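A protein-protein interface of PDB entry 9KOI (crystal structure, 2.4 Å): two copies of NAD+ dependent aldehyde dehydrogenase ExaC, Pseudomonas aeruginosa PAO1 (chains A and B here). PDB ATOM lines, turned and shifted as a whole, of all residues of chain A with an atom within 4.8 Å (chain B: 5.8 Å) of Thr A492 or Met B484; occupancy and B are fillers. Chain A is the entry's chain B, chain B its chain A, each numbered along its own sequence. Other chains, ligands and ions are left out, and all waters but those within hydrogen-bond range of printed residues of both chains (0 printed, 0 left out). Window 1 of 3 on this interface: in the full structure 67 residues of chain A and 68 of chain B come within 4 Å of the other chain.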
ATOM      1  N   HIS A 151      -7.805 -16.980 -27.239  1.00  0.00           N
ATOM      2  CA  HIS A 151      -8.966 -16.136 -26.989  1.00  0.00           C
ATOM      3  C   HIS A 151     -10.131 -16.688 -27.797  1.00  0.00           C
ATOM      4  O   HIS A 151     -10.050 -16.774 -29.026  1.00  0.00           O
ATOM      5  CB  HIS A 151      -8.683 -14.681 -27.365  1.00  0.00           C
ATOM      6  CG  HIS A 151      -7.587 -14.054 -26.562  1.00  0.00           C
ATOM      7  ND1 HIS A 151      -6.271 -14.057 -26.970  1.00  0.00           N
ATOM      8  CD2 HIS A 151      -7.611 -13.411 -25.373  1.00  0.00           C
ATOM      9  CE1 HIS A 151      -5.532 -13.437 -26.068  1.00  0.00           C
ATOM     10  NE2 HIS A 151      -6.321 -13.035 -25.089  1.00  0.00           N
ATOM     11  N   ILE A 152     -11.203 -17.068 -27.108  1.00  0.00           N
ATOM     12  CA  ILE A 152     -12.370 -17.675 -27.735  1.00  0.00           C
ATOM     13  C   ILE A 152     -13.579 -16.802 -27.441  1.00  0.00           C
ATOM     14  O   ILE A 152     -13.879 -16.518 -26.275  1.00  0.00           O
ATOM     15  CB  ILE A 152     -12.604 -19.113 -27.247  1.00  0.00           C
ATOM     16  CG1 ILE A 152     -11.397 -19.992 -27.577  1.00  0.00           C
ATOM     17  CG2 ILE A 152     -13.864 -19.685 -27.874  1.00  0.00           C
ATOM     18  CD1 ILE A 152     -11.553 -21.426 -27.125  1.00  0.00           C
ATOM     19  N   GLN A 490     -20.620 -10.571 -26.655  1.00  0.00           N
ATOM     20  CA  GLN A 490     -19.813 -11.735 -26.330  1.00  0.00           C
ATOM     21  C   GLN A 490     -18.741 -11.314 -25.336  1.00  0.00           C
ATOM     22  O   GLN A 490     -18.425 -10.129 -25.204  1.00  0.00           O
ATOM     23  CB  GLN A 490     -19.160 -12.347 -27.579  1.00  0.00           C
ATOM     24  CG  GLN A 490     -20.133 -12.988 -28.550  1.00  0.00           C
ATOM     25  CD  GLN A 490     -19.467 -13.420 -29.840  1.00  0.00           C
ATOM     26  OE1 GLN A 490     -18.805 -12.625 -30.506  1.00  0.00           O
ATOM     27  NE2 GLN A 490     -19.640 -14.686 -30.201  1.00  0.00           N
ATOM     28  N   GLN A 491     -18.186 -12.294 -24.627  1.00  0.00           N
ATOM     29  CA  GLN A 491     -17.014 -12.060 -23.798  1.00  0.00           C
ATOM     30  C   GLN A 491     -15.858 -12.935 -24.257  1.00  0.00           C
ATOM     31  O   GLN A 491     -16.050 -14.041 -24.772  1.00  0.00           O
ATOM     32  CB  GLN A 491     -17.285 -12.304 -22.308  1.00  0.00           C
ATOM     33  CG  GLN A 491     -18.321 -13.352 -21.981  1.00  0.00           C
ATOM     34  CD  GLN A 491     -18.804 -13.221 -20.550  1.00  0.00           C
ATOM     35  OE1 GLN A 491     -18.656 -12.165 -19.933  1.00  0.00           O
ATOM     36  NE2 GLN A 491     -19.392 -14.285 -20.019  1.00  0.00           N
ATOM     37  N   THR A 492     -14.651 -12.410 -24.067  1.00  0.00           N
ATOM     38  CA  THR A 492     -13.423 -13.083 -24.464  1.00  0.00           C
ATOM     39  C   THR A 492     -12.964 -13.994 -23.335  1.00  0.00           C
ATOM     40  O   THR A 492     -12.675 -13.523 -22.229  1.00  0.00           O
ATOM     41  CB  THR A 492     -12.333 -12.067 -24.795  1.00  0.00           C
ATOM     42  OG1 THR A 492     -12.768 -11.220 -25.865  1.00  0.00           O
ATOM     43  CG2 THR A 492     -11.046 -12.776 -25.195  1.00  0.00           C
ATOM     44  N   LYS A 493     -12.911 -15.292 -23.606  1.00  0.00           N
ATOM     45  CA  LYS A 493     -12.322 -16.248 -22.683  1.00  0.00           C
ATOM     46  C   LYS A 493     -10.876 -16.505 -23.077  1.00  0.00           C
ATOM     47  O   LYS A 493     -10.605 -17.032 -24.162  1.00  0.00           O
ATOM     48  CB  LYS A 493     -13.090 -17.562 -22.656  1.00  0.00           C
ATOM     49  CG  LYS A 493     -12.330 -18.631 -21.910  1.00  0.00           C
ATOM     50  CD  LYS A 493     -13.242 -19.741 -21.524  1.00  0.00           C
ATOM     51  CE  LYS A 493     -14.104 -19.324 -20.360  1.00  0.00           C
ATOM     52  NZ  LYS A 493     -15.240 -20.264 -20.193  1.00  0.00           N
ATOM     53  N   ASN A 494      -9.955 -16.133 -22.197  1.00  0.00           N
ATOM     54  CA  ASN A 494      -8.540 -16.389 -22.414  1.00  0.00           C
ATOM     55  C   ASN A 494      -8.171 -17.732 -21.797  1.00  0.00           C
ATOM     56  O   ASN A 494      -8.257 -17.906 -20.577  1.00  0.00           O
ATOM     57  CB  ASN A 494      -7.681 -15.277 -21.821  1.00  0.00           C
ATOM     58  CG  ASN A 494      -6.203 -15.496 -22.070  1.00  0.00           C
ATOM     59  OD1 ASN A 494      -5.752 -15.490 -23.216  1.00  0.00           O
ATOM     60  ND2 ASN A 494      -5.442 -15.700 -21.002  1.00  0.00           N
ATOM     61  N   TYR B 128       5.499  -3.519 -24.761  1.00  0.00           N
ATOM     62  CA  TYR B 128       4.404  -4.182 -25.463  1.00  0.00           C
ATOM     63  C   TYR B 128       3.472  -3.172 -26.123  1.00  0.00           C
ATOM     64  O   TYR B 128       3.101  -3.326 -27.292  1.00  0.00           O
ATOM     65  CB  TYR B 128       3.625  -5.069 -24.490  1.00  0.00           C
ATOM     66  CG  TYR B 128       2.349  -5.643 -25.064  1.00  0.00           C
ATOM     67  CD1 TYR B 128       2.384  -6.671 -25.996  1.00  0.00           C
ATOM     68  CD2 TYR B 128       1.108  -5.146 -24.681  1.00  0.00           C
ATOM     69  CE1 TYR B 128       1.221  -7.196 -26.525  1.00  0.00           C
ATOM     70  CE2 TYR B 128      -0.062  -5.664 -25.207  1.00  0.00           C
ATOM     71  CZ  TYR B 128       0.002  -6.689 -26.128  1.00  0.00           C
ATOM     72  OH  TYR B 128      -1.157  -7.211 -26.658  1.00  0.00           O
ATOM     73  N   ALA B 452     -14.992 -17.772 -16.172  1.00  0.00           N
ATOM     74  CA  ALA B 452     -13.985 -16.816 -15.747  1.00  0.00           C
ATOM     75  C   ALA B 452     -13.292 -16.257 -16.979  1.00  0.00           C
ATOM     76  O   ALA B 452     -13.195 -16.926 -18.013  1.00  0.00           O
ATOM     77  CB  ALA B 452     -12.957 -17.453 -14.802  1.00  0.00           C
ATOM     78  N   GLY B 453     -12.799 -15.024 -16.857  1.00  0.00           N
ATOM     79  CA  GLY B 453     -12.140 -14.391 -17.987  1.00  0.00           C
ATOM     80  C   GLY B 453     -10.855 -15.090 -18.380  1.00  0.00           C
ATOM     81  O   GLY B 453     -10.529 -15.191 -19.566  1.00  0.00           O
ATOM     82  N   ALA B 468      -5.515 -11.505 -22.818  1.00  0.00           N
ATOM     83  CA  ALA B 468      -6.598 -10.691 -22.279  1.00  0.00           C
ATOM     84  C   ALA B 468      -6.886 -11.052 -20.829  1.00  0.00           C
ATOM     85  O   ALA B 468      -7.070 -12.224 -20.489  1.00  0.00           O
ATOM     86  CB  ALA B 468      -7.859 -10.863 -23.122  1.00  0.00           C
ATOM     87  N   TYR B 472     -15.529 -11.986 -15.700  1.00  0.00           N
ATOM     88  CA  TYR B 472     -16.940 -12.298 -15.870  1.00  0.00           C
ATOM     89  C   TYR B 472     -17.717 -11.823 -14.647  1.00  0.00           C
ATOM     90  O   TYR B 472     -17.140 -11.411 -13.641  1.00  0.00           O
ATOM     91  CB  TYR B 472     -17.156 -13.801 -16.060  1.00  0.00           C
ATOM     92  CG  TYR B 472     -16.777 -14.381 -17.407  1.00  0.00           C
ATOM     93  CD1 TYR B 472     -15.882 -13.739 -18.255  1.00  0.00           C
ATOM     94  CD2 TYR B 472     -17.336 -15.577 -17.833  1.00  0.00           C
ATOM     95  CE1 TYR B 472     -15.548 -14.288 -19.485  1.00  0.00           C
ATOM     96  CE2 TYR B 472     -17.010 -16.131 -19.051  1.00  0.00           C
ATOM     97  CZ  TYR B 472     -16.119 -15.485 -19.876  1.00  0.00           C
ATOM     98  OH  TYR B 472     -15.804 -16.043 -21.092  1.00  0.00           O
ATOM     99  N   ARG B 479     -11.176  -5.656 -20.520  1.00  0.00           N
ATOM    100  CA  ARG B 479     -10.002  -6.516 -20.521  1.00  0.00           C
ATOM    101  C   ARG B 479      -8.741  -5.675 -20.368  1.00  0.00           C
ATOM    102  O   ARG B 479      -8.705  -4.511 -20.778  1.00  0.00           O
ATOM    103  CB  ARG B 479      -9.914  -7.329 -21.816  1.00  0.00           C
ATOM    104  CG  ARG B 479     -11.014  -8.356 -21.985  1.00  0.00           C
ATOM    105  CD  ARG B 479     -10.932  -9.411 -20.904  1.00  0.00           C
ATOM    106  NE  ARG B 479     -11.921 -10.464 -21.088  1.00  0.00           N
ATOM    107  CZ  ARG B 479     -13.117 -10.477 -20.518  1.00  0.00           C
ATOM    108  NH1 ARG B 479     -13.517  -9.492 -19.731  1.00  0.00           N
ATOM    109  NH2 ARG B 479     -13.932 -11.504 -20.742  1.00  0.00           N
ATOM    110  N   HIS B 482      -3.710  -6.593 -22.837  1.00  0.00           N
ATOM    111  CA  HIS B 482      -3.827  -7.047 -24.215  1.00  0.00           C
ATOM    112  C   HIS B 482      -4.120  -5.841 -25.095  1.00  0.00           C
ATOM    113  O   HIS B 482      -4.633  -4.824 -24.631  1.00  0.00           O
ATOM    114  CB  HIS B 482      -4.908  -8.126 -24.372  1.00  0.00           C
ATOM    115  CG  HIS B 482      -4.957  -8.741 -25.737  1.00  0.00           C
ATOM    116  ND1 HIS B 482      -5.816  -8.306 -26.720  1.00  0.00           N
ATOM    117  CD2 HIS B 482      -4.256  -9.765 -26.280  1.00  0.00           C
ATOM    118  CE1 HIS B 482      -5.646  -9.030 -27.811  1.00  0.00           C
ATOM    119  NE2 HIS B 482      -4.703  -9.923 -27.570  1.00  0.00           N
ATOM    120  N   LYS B 483      -3.786  -5.965 -26.379  1.00  0.00           N
ATOM    121  CA  LYS B 483      -3.932  -4.843 -27.298  1.00  0.00           C
ATOM    122  C   LYS B 483      -5.382  -4.426 -27.523  1.00  0.00           C
ATOM    123  O   LYS B 483      -5.622  -3.284 -27.934  1.00  0.00           O
ATOM    124  CB  LYS B 483      -3.278  -5.176 -28.637  1.00  0.00           C
ATOM    125  CG  LYS B 483      -3.956  -6.298 -29.389  1.00  0.00           C
ATOM    126  CD  LYS B 483      -3.257  -6.556 -30.711  1.00  0.00           C
ATOM    127  CE  LYS B 483      -4.041  -7.545 -31.554  1.00  0.00           C
ATOM    128  NZ  LYS B 483      -3.440  -7.730 -32.900  1.00  0.00           N
ATOM    129  N   MET B 484      -6.355  -5.308 -27.270  1.00  0.00           N
ATOM    130  CA  MET B 484      -7.760  -4.924 -27.423  1.00  0.00           C
ATOM    131  C   MET B 484      -8.181  -3.800 -26.483  1.00  0.00           C
ATOM    132  O   MET B 484      -9.271  -3.246 -26.664  1.00  0.00           O
ATOM    133  CB  MET B 484      -8.678  -6.132 -27.215  1.00  0.00           C
ATOM    134  CG  MET B 484      -8.436  -6.917 -25.940  1.00  0.00           C
ATOM    135  SD  MET B 484      -9.905  -7.792 -25.373  1.00  0.00           S
ATOM    136  CE  MET B 484      -9.539  -9.449 -25.939  1.00  0.00           C
ATOM    137  N   MET B 485      -7.363  -3.462 -25.479  1.00  0.00           N
ATOM    138  CA  MET B 485      -7.716  -2.359 -24.591  1.00  0.00           C
ATOM    139  C   MET B 485      -7.739  -1.036 -25.336  1.00  0.00           C
ATOM    140  O   MET B 485      -8.548  -0.158 -25.018  1.00  0.00           O
ATOM    141  CB  MET B 485      -6.730  -2.251 -23.429  1.00  0.00           C
ATOM    142  CG  MET B 485      -6.453  -3.510 -22.667  1.00  0.00           C
ATOM    143  SD  MET B 485      -4.990  -3.227 -21.659  1.00  0.00           S
ATOM    144  CE  MET B 485      -5.573  -1.871 -20.644  1.00  0.00           C
ATOM    145  N   LEU B 486      -6.843  -0.868 -26.316  1.00  0.00           N
ATOM    146  CA  LEU B 486      -6.694   0.420 -26.995  1.00  0.00           C
ATOM    147  C   LEU B 486      -8.038   1.013 -27.398  1.00  0.00           C
ATOM    148  O   LEU B 486      -8.225   2.235 -27.361  1.00  0.00           O
ATOM    149  CB  LEU B 486      -5.787   0.260 -28.217  1.00  0.00           C
ATOM    150  CG  LEU B 486      -4.308   0.000 -27.916  1.00  0.00           C
ATOM    151  CD1 LEU B 486      -3.524  -0.218 -29.201  1.00  0.00           C
ATOM    152  CD2 LEU B 486      -3.713   1.143 -27.105  1.00  0.00           C
ATOM    153  N   ASP B 487      -8.991   0.160 -27.779  1.00  0.00           N
ATOM    154  CA  ASP B 487     -10.334   0.629 -28.094  1.00  0.00           C
ATOM    155  C   ASP B 487     -11.072   1.161 -26.866  1.00  0.00           C
ATOM    156  O   ASP B 487     -12.088   1.845 -27.025  1.00  0.00           O
ATOM    157  CB  ASP B 487     -11.128  -0.495 -28.759  1.00  0.00           C
ATOM    158  CG  ASP B 487     -10.384  -1.110 -29.931  1.00  0.00           C
ATOM    159  OD1 ASP B 487     -10.675  -2.270 -30.288  1.00  0.00           O
ATOM    160  OD2 ASP B 487      -9.504  -0.425 -30.497  1.00  0.00           O
ATOM    161  N   HIS B 488     -10.599   0.863 -25.650  1.00  0.00           N
ATOM    162  CA  HIS B 488     -11.182   1.479 -24.462  1.00  0.00           C
ATOM    163  C   HIS B 488     -10.630   2.874 -24.214  1.00  0.00           C
ATOM    164  O   HIS B 488     -11.290   3.681 -23.553  1.00  0.00           O
ATOM    165  CB  HIS B 488     -10.934   0.631 -23.208  1.00  0.00           C
ATOM    166  CG  HIS B 488     -11.778  -0.601 -23.120  1.00  0.00           C
ATOM    167  ND1 HIS B 488     -11.239  -1.865 -23.005  1.00  0.00           N
ATOM    168  CD2 HIS B 488     -13.121  -0.767 -23.120  1.00  0.00           C
ATOM    169  CE1 HIS B 488     -12.212  -2.755 -22.938  1.00  0.00           C
ATOM    170  NE2 HIS B 488     -13.366  -2.115 -23.007  1.00  0.00           N
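Among the printed residues, merely in contact across the chains: His A151 with His B482 (3.9 Å), Gln A491 with Tyr B472 (3.2 Å), Gln A491 with Arg B479 (3.8 Å), Thr A492 with Gly B453 (3.8 Å), Thr A492 with Met B484 (3.7 Å), Lys A493 with Ala B452 (3.5 Å), Lys A493 with Gly B453 (3.7 Å), Lys A493 with Tyr B472 (3.5 Å) and Asn A494 with Ala B468 (3.4 Å).
Thr A492 touches just these residues of chain B: Gly B453, Arg B479 and Met B484. Met B484 touches just one residue of chain A: Thr A492 (3.7 Å). Of the printed residues of chain A, His B482 touches His A151. Printed residues of chain A within 4 Å of Arg B479: Gln A491 and Thr A492. Of the printed residues of chain A, Ala B468 touches His A151 and Asn A494. Printed residues of chain B within 4 Å of Asn A494: Gly B453 and Ala B468. Printed residues of chain B within 4 Å of His A151: Ala B468 and His B482. Met B485 touches none of the printed residues of chain A. The nearest residue of chain A that does not touch Met B484 is His A151 (4.4 Å). The nearest printed residue of chain A that does not touch Tyr B472 is Thr A492 (4.05 Å).
No position is printed for both chains. Of the 12 pairs that touch across the chains among the printed residues, none has its exchanged pair printed and touching as well.
A ring nitrogen (ND1) of His B482 sits close to the backbone NH (N) of Met B484. The backbone NH (N) of His B482 lies within hydrogen-bond range of the side-chain sulfur (SD) of Met B485. A ring nitrogen (NE2) of His A151 is in hydrogen-bond range of the side-chain amide oxygen (OD1) of Asn A494 (3.1 Å). O of Lys A493 sits at hydrogen-bond distance from N of Ile A152, at 3.0 Å.
Of the 7 printed residues of chain A, 5 touch a printed residue of chain B. Hydrophobic or aromatic side chains of chain A within 4 Å of the printed part of chain B: His A151. Of the 13 printed residues of chain B, 7 touch a printed residue of chain A. Printed residues of chain B that touch a printed residue of chain A: Ala B452, Gly B453, Ala B468, Tyr B472, Arg B479, His B482 and Met B484. Hydrophobic or aromatic side chains of chain B within 4 Å of the printed part of chain A: Ala B468, Tyr B472, His B482 and Met B484. Among the printed residues, 12 pairs touch across the chains.
N of Asn A494 sits at hydrogen-bond distance from O of Gly B453. N of Ala B468 is in hydrogen-bond range of NE2 of His A151 (2.9 Å). The guanidinium group of Arg B479 sits at hydrogen-bond distance from the backbone carbonyl oxygen of Thr A492, 2.8 Å away.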
